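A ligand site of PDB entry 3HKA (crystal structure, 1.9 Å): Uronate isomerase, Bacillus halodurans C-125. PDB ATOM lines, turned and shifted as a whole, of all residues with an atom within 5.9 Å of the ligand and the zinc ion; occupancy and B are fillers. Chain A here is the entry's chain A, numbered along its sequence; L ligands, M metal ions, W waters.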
ATOM      1  N   HIS A  26      11.088 -20.182  26.151  1.00  0.00           N
ATOM      2  CA  HIS A  26      12.466 -20.628  25.954  1.00  0.00           C
ATOM      3  C   HIS A  26      12.736 -21.998  26.557  1.00  0.00           C
ATOM      4  O   HIS A  26      12.755 -22.157  27.773  1.00  0.00           O
ATOM      5  CB  HIS A  26      13.522 -19.653  26.490  1.00  0.00           C
ATOM      6  CG  HIS A  26      14.919 -20.180  26.337  1.00  0.00           C
ATOM      7  ND1 HIS A  26      15.445 -20.557  25.117  1.00  0.00           N
ATOM      8  CD2 HIS A  26      15.860 -20.485  27.264  1.00  0.00           C
ATOM      9  CE1 HIS A  26      16.651 -21.078  25.298  1.00  0.00           C
ATOM     10  NE2 HIS A  26      16.922 -21.043  26.590  1.00  0.00           N
ATOM     11  N   THR A  27      12.944 -22.983  25.690  1.00  0.00           N
ATOM     12  CA  THR A  27      13.236 -24.337  26.135  1.00  0.00           C
ATOM     13  C   THR A  27      14.214 -24.944  25.139  1.00  0.00           C
ATOM     14  O   THR A  27      14.536 -24.332  24.118  1.00  0.00           O
ATOM     15  CB  THR A  27      11.994 -25.255  26.129  1.00  0.00           C
ATOM     16  OG1 THR A  27      11.735 -25.705  24.791  1.00  0.00           O
ATOM     17  CG2 THR A  27      10.774 -24.507  26.665  1.00  0.00           C
ATOM     18  N   HIS A  28      14.649 -26.151  25.454  1.00  0.00           N
ATOM     19  CA  HIS A  28      15.547 -26.880  24.588  1.00  0.00           C
ATOM     20  C   HIS A  28      14.849 -28.194  24.229  1.00  0.00           C
ATOM     21  O   HIS A  28      15.454 -29.263  24.180  1.00  0.00           O
ATOM     22  CB  HIS A  28      16.874 -27.142  25.314  1.00  0.00           C
ATOM     23  CG  HIS A  28      17.681 -25.890  25.499  1.00  0.00           C
ATOM     24  ND1 HIS A  28      18.539 -25.412  24.525  1.00  0.00           N
ATOM     25  CD2 HIS A  28      17.720 -24.998  26.505  1.00  0.00           C
ATOM     26  CE1 HIS A  28      19.061 -24.278  24.932  1.00  0.00           C
ATOM     27  NE2 HIS A  28      18.579 -23.995  26.128  1.00  0.00           N
ATOM     28  N   TYR A  48      20.575 -34.966  33.478  1.00  0.00           N
ATOM     29  CA  TYR A  48      20.488 -33.535  33.148  1.00  0.00           C
ATOM     30  C   TYR A  48      21.840 -32.977  33.589  1.00  0.00           C
ATOM     31  O   TYR A  48      22.331 -33.341  34.643  1.00  0.00           O
ATOM     32  CB  TYR A  48      19.346 -32.942  33.985  1.00  0.00           C
ATOM     33  CG  TYR A  48      19.067 -31.461  33.866  1.00  0.00           C
ATOM     34  CD1 TYR A  48      19.116 -30.807  32.635  1.00  0.00           C
ATOM     35  CD2 TYR A  48      18.620 -30.752  34.969  1.00  0.00           C
ATOM     36  CE1 TYR A  48      18.715 -29.470  32.520  1.00  0.00           C
ATOM     37  CE2 TYR A  48      18.208 -29.421  34.873  1.00  0.00           C
ATOM     38  CZ  TYR A  48      18.257 -28.788  33.642  1.00  0.00           C
ATOM     39  OH  TYR A  48      17.825 -27.488  33.553  1.00  0.00           O
ATOM     40  N   HIS A  49      22.456 -32.098  32.787  1.00  0.00           N
ATOM     41  CA  HIS A  49      23.775 -31.601  33.183  1.00  0.00           C
ATOM     42  C   HIS A  49      23.865 -30.942  34.556  1.00  0.00           C
ATOM     43  O   HIS A  49      24.930 -30.958  35.170  1.00  0.00           O
ATOM     44  CB  HIS A  49      24.418 -30.735  32.075  1.00  0.00           C
ATOM     45  CG  HIS A  49      23.848 -29.354  31.929  1.00  0.00           C
ATOM     46  ND1 HIS A  49      24.081 -28.349  32.844  1.00  0.00           N
ATOM     47  CD2 HIS A  49      23.117 -28.801  30.932  1.00  0.00           C
ATOM     48  CE1 HIS A  49      23.532 -27.221  32.404  1.00  0.00           C
ATOM     49  NE2 HIS A  49      22.940 -27.475  31.251  1.00  0.00           N
ATOM     50  N   TYR A  50      22.753 -30.406  35.056  1.00  0.00           N
ATOM     51  CA  TYR A  50      22.762 -29.793  36.386  1.00  0.00           C
ATOM     52  C   TYR A  50      23.170 -30.853  37.402  1.00  0.00           C
ATOM     53  O   TYR A  50      23.928 -30.581  38.339  1.00  0.00           O
ATOM     54  CB  TYR A  50      21.362 -29.311  36.777  1.00  0.00           C
ATOM     55  CG  TYR A  50      20.960 -27.961  36.213  1.00  0.00           C
ATOM     56  CD1 TYR A  50      21.244 -27.619  34.902  1.00  0.00           C
ATOM     57  CD2 TYR A  50      20.204 -27.077  36.983  1.00  0.00           C
ATOM     58  CE1 TYR A  50      20.782 -26.430  34.358  1.00  0.00           C
ATOM     59  CE2 TYR A  50      19.741 -25.883  36.456  1.00  0.00           C
ATOM     60  CZ  TYR A  50      20.033 -25.564  35.139  1.00  0.00           C
ATOM     61  OH  TYR A  50      19.535 -24.409  34.598  1.00  0.00           O
ATOM     62  N   THR A 143      14.616 -24.024  20.732  1.00  0.00           N
ATOM     63  CA  THR A 143      15.878 -23.355  20.460  1.00  0.00           C
ATOM     64  C   THR A 143      16.341 -24.084  19.207  1.00  0.00           C
ATOM     65  O   THR A 143      16.819 -25.220  19.274  1.00  0.00           O
ATOM     66  CB  THR A 143      16.904 -23.563  21.573  1.00  0.00           C
ATOM     67  OG1 THR A 143      16.443 -22.928  22.777  1.00  0.00           O
ATOM     68  CG2 THR A 143      18.256 -22.979  21.169  1.00  0.00           C
ATOM     69  N   ARG A 170      18.240 -19.659  16.748  1.00  0.00           N
ATOM     70  CA  ARG A 170      19.413 -19.512  17.615  1.00  0.00           C
ATOM     71  C   ARG A 170      20.650 -19.296  16.729  1.00  0.00           C
ATOM     72  O   ARG A 170      20.893 -20.075  15.806  1.00  0.00           O
ATOM     73  CB  ARG A 170      19.579 -20.760  18.483  1.00  0.00           C
ATOM     74  CG  ARG A 170      20.651 -20.646  19.553  1.00  0.00           C
ATOM     75  CD  ARG A 170      20.387 -19.478  20.510  1.00  0.00           C
ATOM     76  NE  ARG A 170      21.395 -19.483  21.561  1.00  0.00           N
ATOM     77  CZ  ARG A 170      21.195 -19.973  22.784  1.00  0.00           C
ATOM     78  NH1 ARG A 170      20.018 -20.470  23.122  1.00  0.00           N
ATOM     79  NH2 ARG A 170      22.198 -20.005  23.639  1.00  0.00           N
ATOM     80  N   ASP A 172      24.167 -18.405  18.029  1.00  0.00           N
ATOM     81  CA  ASP A 172      25.471 -18.329  18.701  1.00  0.00           C
ATOM     82  C   ASP A 172      26.682 -18.568  17.784  1.00  0.00           C
ATOM     83  O   ASP A 172      27.652 -17.808  17.807  1.00  0.00           O
ATOM     84  CB  ASP A 172      25.514 -19.307  19.876  1.00  0.00           C
ATOM     85  CG  ASP A 172      24.592 -18.878  21.006  1.00  0.00           C
ATOM     86  OD1 ASP A 172      23.541 -18.278  20.712  1.00  0.00           O
ATOM     87  OD2 ASP A 172      24.914 -19.173  22.183  1.00  0.00           O
ATOM     88  N   SER A 223      23.207 -16.282  23.058  1.00  0.00           N
ATOM     89  CA  SER A 223      23.636 -16.204  24.448  1.00  0.00           C
ATOM     90  C   SER A 223      24.976 -15.482  24.338  1.00  0.00           C
ATOM     91  O   SER A 223      25.733 -15.728  23.404  1.00  0.00           O
ATOM     92  CB  SER A 223      23.791 -17.608  25.082  1.00  0.00           C
ATOM     93  OG  SER A 223      24.894 -18.321  24.554  1.00  0.00           O
ATOM     94  N   MET A 258      20.656 -13.452  25.798  1.00  0.00           N
ATOM     95  CA  MET A 258      20.799 -14.104  27.090  1.00  0.00           C
ATOM     96  C   MET A 258      22.255 -13.820  27.457  1.00  0.00           C
ATOM     97  O   MET A 258      23.187 -14.486  26.998  1.00  0.00           O
ATOM     98  CB  MET A 258      20.503 -15.597  26.954  1.00  0.00           C
ATOM     99  CG  MET A 258      19.219 -15.837  26.174  1.00  0.00           C
ATOM    100  SD  MET A 258      18.401 -17.404  26.512  1.00  0.00           S
ATOM    101  CE  MET A 258      19.229 -18.453  25.415  1.00  0.00           C
ATOM    102  N   LYS A 263      31.402 -19.492  28.694  1.00  0.00           N
ATOM    103  CA  LYS A 263      31.453 -20.862  28.199  1.00  0.00           C
ATOM    104  C   LYS A 263      32.697 -21.676  28.507  1.00  0.00           C
ATOM    105  O   LYS A 263      33.823 -21.166  28.493  1.00  0.00           O
ATOM    106  CB  LYS A 263      31.252 -20.853  26.678  1.00  0.00           C
ATOM    107  CG  LYS A 263      29.946 -20.213  26.216  1.00  0.00           C
ATOM    108  CD  LYS A 263      28.719 -20.998  26.677  1.00  0.00           C
ATOM    109  CE  LYS A 263      28.561 -22.312  25.922  1.00  0.00           C
ATOM    110  NZ  LYS A 263      27.300 -23.023  26.317  1.00  0.00           N
ATOM    111  N   ASP A 271      28.398 -29.843  28.791  1.00  0.00           N
ATOM    112  CA  ASP A 271      27.364 -28.838  29.016  1.00  0.00           C
ATOM    113  C   ASP A 271      27.260 -28.377  30.465  1.00  0.00           C
ATOM    114  O   ASP A 271      26.561 -27.409  30.764  1.00  0.00           O
ATOM    115  CB  ASP A 271      25.987 -29.342  28.573  1.00  0.00           C
ATOM    116  CG  ASP A 271      25.869 -29.514  27.068  1.00  0.00           C
ATOM    117  OD1 ASP A 271      26.640 -28.874  26.333  1.00  0.00           O
ATOM    118  OD2 ASP A 271      24.989 -30.285  26.639  1.00  0.00           O
ATOM    119  N   ASP A 274      29.888 -24.648  32.082  1.00  0.00           N
ATOM    120  CA  ASP A 274      29.765 -23.208  31.839  1.00  0.00           C
ATOM    121  C   ASP A 274      29.663 -22.445  33.166  1.00  0.00           C
ATOM    122  O   ASP A 274      29.125 -22.953  34.157  1.00  0.00           O
ATOM    123  CB  ASP A 274      28.550 -22.892  30.959  1.00  0.00           C
ATOM    124  CG  ASP A 274      28.664 -23.480  29.559  1.00  0.00           C
ATOM    125  OD1 ASP A 274      29.792 -23.604  29.041  1.00  0.00           O
ATOM    126  OD2 ASP A 274      27.604 -23.800  28.957  1.00  0.00           O
ATOM    127  N   TRP A 325      16.858 -17.175  34.503  1.00  0.00           N
ATOM    128  CA  TRP A 325      17.747 -18.054  33.781  1.00  0.00           C
ATOM    129  C   TRP A 325      18.861 -18.824  34.474  1.00  0.00           C
ATOM    130  O   TRP A 325      19.686 -18.263  35.192  1.00  0.00           O
ATOM    131  CB  TRP A 325      18.350 -17.231  32.617  1.00  0.00           C
ATOM    132  CG  TRP A 325      19.166 -18.009  31.637  1.00  0.00           C
ATOM    133  CD1 TRP A 325      18.923 -19.269  31.159  1.00  0.00           C
ATOM    134  CD2 TRP A 325      20.329 -17.531  30.936  1.00  0.00           C
ATOM    135  NE1 TRP A 325      19.841 -19.598  30.195  1.00  0.00           N
ATOM    136  CE2 TRP A 325      20.723 -18.551  30.039  1.00  0.00           C
ATOM    137  CE3 TRP A 325      21.063 -16.336  30.967  1.00  0.00           C
ATOM    138  CZ2 TRP A 325      21.824 -18.408  29.187  1.00  0.00           C
ATOM    139  CZ3 TRP A 325      22.156 -16.193  30.121  1.00  0.00           C
ATOM    140  CH2 TRP A 325      22.526 -17.236  29.242  1.00  0.00           C
ATOM    141  N   TRP A 326      18.852 -20.135  34.255  1.00  0.00           N
ATOM    142  CA  TRP A 326      19.920 -21.011  34.730  1.00  0.00           C
ATOM    143  C   TRP A 326      20.263 -20.929  36.225  1.00  0.00           C
ATOM    144  O   TRP A 326      19.504 -21.398  37.079  1.00  0.00           O
ATOM    145  CB  TRP A 326      21.147 -20.644  33.896  1.00  0.00           C
ATOM    146  CG  TRP A 326      22.145 -21.718  33.622  1.00  0.00           C
ATOM    147  CD1 TRP A 326      22.423 -22.810  34.388  1.00  0.00           C
ATOM    148  CD2 TRP A 326      23.076 -21.736  32.534  1.00  0.00           C
ATOM    149  NE1 TRP A 326      23.484 -23.522  33.836  1.00  0.00           N
ATOM    150  CE2 TRP A 326      23.897 -22.878  32.702  1.00  0.00           C
ATOM    151  CE3 TRP A 326      23.293 -20.896  31.432  1.00  0.00           C
ATOM    152  CZ2 TRP A 326      24.919 -23.198  31.796  1.00  0.00           C
ATOM    153  CZ3 TRP A 326      24.319 -21.220  30.534  1.00  0.00           C
ATOM    154  CH2 TRP A 326      25.113 -22.367  30.732  1.00  0.00           C
ATOM    155  N   HIS A 353      10.548 -18.961  32.348  1.00  0.00           N
ATOM    156  CA  HIS A 353      10.617 -19.898  31.236  1.00  0.00           C
ATOM    157  C   HIS A 353      11.247 -21.139  31.878  1.00  0.00           C
ATOM    158  O   HIS A 353      11.897 -21.028  32.924  1.00  0.00           O
ATOM    159  CB  HIS A 353      11.477 -19.363  30.076  1.00  0.00           C
ATOM    160  CG  HIS A 353      12.934 -19.239  30.394  1.00  0.00           C
ATOM    161  ND1 HIS A 353      13.483 -18.095  30.941  1.00  0.00           N
ATOM    162  CD2 HIS A 353      13.957 -20.096  30.203  1.00  0.00           C
ATOM    163  CE1 HIS A 353      14.783 -18.263  31.078  1.00  0.00           C
ATOM    164  NE2 HIS A 353      15.095 -19.466  30.635  1.00  0.00           N
ATOM    165  N   SER A 354      11.065 -22.308  31.277  1.00  0.00           N
ATOM    166  CA  SER A 354      11.606 -23.537  31.879  1.00  0.00           C
ATOM    167  C   SER A 354      13.017 -23.911  31.468  1.00  0.00           C
ATOM    168  O   SER A 354      13.770 -24.482  32.256  1.00  0.00           O
ATOM    169  CB  SER A 354      10.687 -24.712  31.572  1.00  0.00           C
ATOM    170  OG  SER A 354      10.781 -25.071  30.211  1.00  0.00           O
ATOM    171  N   ASP A 355      13.387 -23.604  30.226  1.00  0.00           N
ATOM    172  CA  ASP A 355      14.701 -23.961  29.714  1.00  0.00           C
ATOM    173  C   ASP A 355      14.819 -25.481  29.728  1.00  0.00           C
ATOM    174  O   ASP A 355      15.914 -26.036  29.755  1.00  0.00           O
ATOM    175  CB  ASP A 355      15.801 -23.384  30.611  1.00  0.00           C
ATOM    176  CG  ASP A 355      16.818 -22.582  29.822  1.00  0.00           C
ATOM    177  OD1 ASP A 355      17.298 -23.079  28.779  1.00  0.00           O
ATOM    178  OD2 ASP A 355      17.134 -21.449  30.249  1.00  0.00           O
ATOM    179  N   ARG A 357      15.304 -29.183  29.029  1.00  0.00           N
ATOM    180  CA  ARG A 357      16.147 -29.937  28.102  1.00  0.00           C
ATOM    181  C   ARG A 357      15.564 -31.339  27.993  1.00  0.00           C
ATOM    182  O   ARG A 357      15.749 -32.030  26.989  1.00  0.00           O
ATOM    183  CB  ARG A 357      17.584 -29.995  28.619  1.00  0.00           C
ATOM    184  CG  ARG A 357      18.424 -28.773  28.247  1.00  0.00           C
ATOM    185  CD  ARG A 357      19.808 -28.841  28.878  1.00  0.00           C
ATOM    186  NE  ARG A 357      20.694 -27.801  28.367  1.00  0.00           N
ATOM    187  CZ  ARG A 357      21.205 -27.806  27.139  1.00  0.00           C
ATOM    188  NH1 ARG A 357      20.918 -28.794  26.302  1.00  0.00           N
ATOM    189  NH2 ARG A 357      22.005 -26.824  26.748  1.00  0.00           N
ATOM    190  N   LYS A 365       9.614 -27.583  36.545  1.00  0.00           N
ATOM    191  CA  LYS A 365       9.996 -26.204  36.252  1.00  0.00           C
ATOM    192  C   LYS A 365       8.819 -25.272  36.518  1.00  0.00           C
ATOM    193  O   LYS A 365       8.950 -24.302  37.274  1.00  0.00           O
ATOM    194  CB  LYS A 365      10.442 -26.064  34.791  1.00  0.00           C
ATOM    195  CG  LYS A 365      11.727 -26.804  34.451  1.00  0.00           C
ATOM    196  CD  LYS A 365      12.969 -26.107  34.993  1.00  0.00           C
ATOM    197  CE  LYS A 365      14.230 -26.780  34.463  1.00  0.00           C
ATOM    198  NZ  LYS A 365      15.498 -26.213  35.026  1.00  0.00           N
HETATM  199  O1  LIG L   1      19.956 -21.445  26.043  1.00  0.00           O
HETATM  200  C1  LIG L   1      21.111 -21.452  26.543  1.00  0.00           C
HETATM  201  O2  LIG L   1      22.148 -21.072  25.976  1.00  0.00           O
HETATM  202  C2  LIG L   1      21.251 -21.963  27.985  1.00  0.00           C
HETATM  203  O3  LIG L   1      19.980 -21.879  28.647  1.00  0.00           O
HETATM  204  C3  LIG L   1      21.796 -23.413  27.993  1.00  0.00           C
HETATM  205  O4  LIG L   1      23.064 -23.433  27.291  1.00  0.00           O
HETATM  206  C4  LIG L   1      22.059 -24.056  29.386  1.00  0.00           C
HETATM  207  O5  LIG L   1      22.848 -25.249  29.251  1.00  0.00           O
HETATM  208  C5  LIG L   1      20.746 -24.411  30.150  1.00  0.00           C
HETATM  209  O6  LIG L   1      19.754 -24.818  29.540  1.00  0.00           O
HETATM  210  C6  LIG L   1      20.684 -24.274  31.662  1.00  0.00           C
HETATM  211  O7  LIG L   1      19.352 -24.104  32.118  1.00  0.00           O
HETATM  212 ZN    ZN M   1      18.503 -22.237  27.341  1.00  0.00          ZN
HETATM  213  O   HOH W   1      25.483 -25.360  29.191  1.00  0.00           O
HETATM  214  O   HOH W   2      18.169 -26.481  31.164  1.00  0.00           O
HETATM  215  O   HOH W   3      24.942 -20.594  26.458  1.00  0.00           O
HETATM  216  O   HOH W   4      16.731 -23.878  34.260  1.00  0.00           O
HETATM  217  O   HOH W   5      23.343 -24.002  24.075  1.00  0.00           O
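An oxygen (O7) of the ligand is in hydrogen-bond range of the side-chain hydroxyl (OH) of Tyr 50 (2.5 Å). NH2 of Arg 170 lies within salt-bridge range of O2 of the ligand. NE1 of Trp 325 lies close to O3 of the ligand (2.8 Å). O5 of the ligand sits at hydrogen-bond distance from NE2 of His 49, at 3.0 Å. The guanidinium group (NH2) of Arg 357 lies within hydrogen-bond range of an oxygen (O5) of the ligand (3.1 Å).
The side-chain carboxylate (OD2) of Asp 355 lies close to the indole nitrogen (NE1) of Trp 325, 3.3 Å away. The side-chain carboxylate (OD2) of Asp 355 sits at hydrogen-bond distance from a ring nitrogen (NE2) of His 353 (2.9 Å). The side-chain hydroxyl of Thr 143 lies close to a ring nitrogen (ND1) of His 26 (3.5 Å). The guanidinium group (NH2) of Arg 170 sits close to the side-chain hydroxyl (OG) of Ser 223 (3.3 Å). The guanidinium group of Arg 170 is in salt-bridge range of the side-chain carboxylate of Asp 172, at 2.6 Å. The backbone carbonyl oxygen (O) of Asp 271 sits at hydrogen-bond distance from a ring nitrogen (ND1) of His 49, 3.4 Å away. OD2 of Asp 172 sits at hydrogen-bond distance from OG of Ser 223, 2.5 Å away. The side-chain hydroxyl (OH) of Tyr 48 lies within hydrogen-bond range of the side-chain amino group (NZ) of Lys 365, 3.0 Å away.
Merely in contact with the ligand: Tyr 48, Ser 223, Met 258 and Trp 326. Hydrophobic or aromatic side chains within 4 Å of the ligand: His 26, His 28, His 49, Tyr 50, Met 258, Trp 325 and Trp 326. The nearest printed residue that does not touch the ligand is Lys 263 (4.4 Å).
O3 of the ligand binds the zinc ion (2.0 Å). The side-chain carboxylate (OD1) of Asp 355 binds the zinc ion (2.1 Å). An oxygen (O1) of the ligand is bound to the zinc ion. NE2 of His 26 is bound to the zinc ion (2.1 Å). NE2 of His 28 is bound to the zinc ion.
Within 4 Å of the zinc ion: His 26, His 28 and Asp 355.
Water W1 lies within hydrogen-bond range of an oxygen (O5) of the ligand (2.6 Å), the side-chain carboxylate (OD2) of Asp 274 (2.6 Å) and the backbone carbonyl oxygen (O) of Asp 271 (2.8 Å). Water W2 lies within hydrogen-bond range of the side-chain hydroxyl (OH) of Tyr 48 (2.6 Å), the backbone carbonyl oxygen (O) of Asp 355 (2.7 Å) and an oxygen (O6) of the ligand (2.8 Å). Water W3 lies within hydrogen-bond range of O2 of the ligand (2.9 Å), OG of Ser 223 (3.0 Å) and NZ of Lys 263 (3.4 Å). Water W4 lies within hydrogen-bond range of the side-chain amino group (NZ) of Lys 365, the side-chain hydroxyl (OH) of Tyr 50 and an oxygen (O7) of the ligand.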
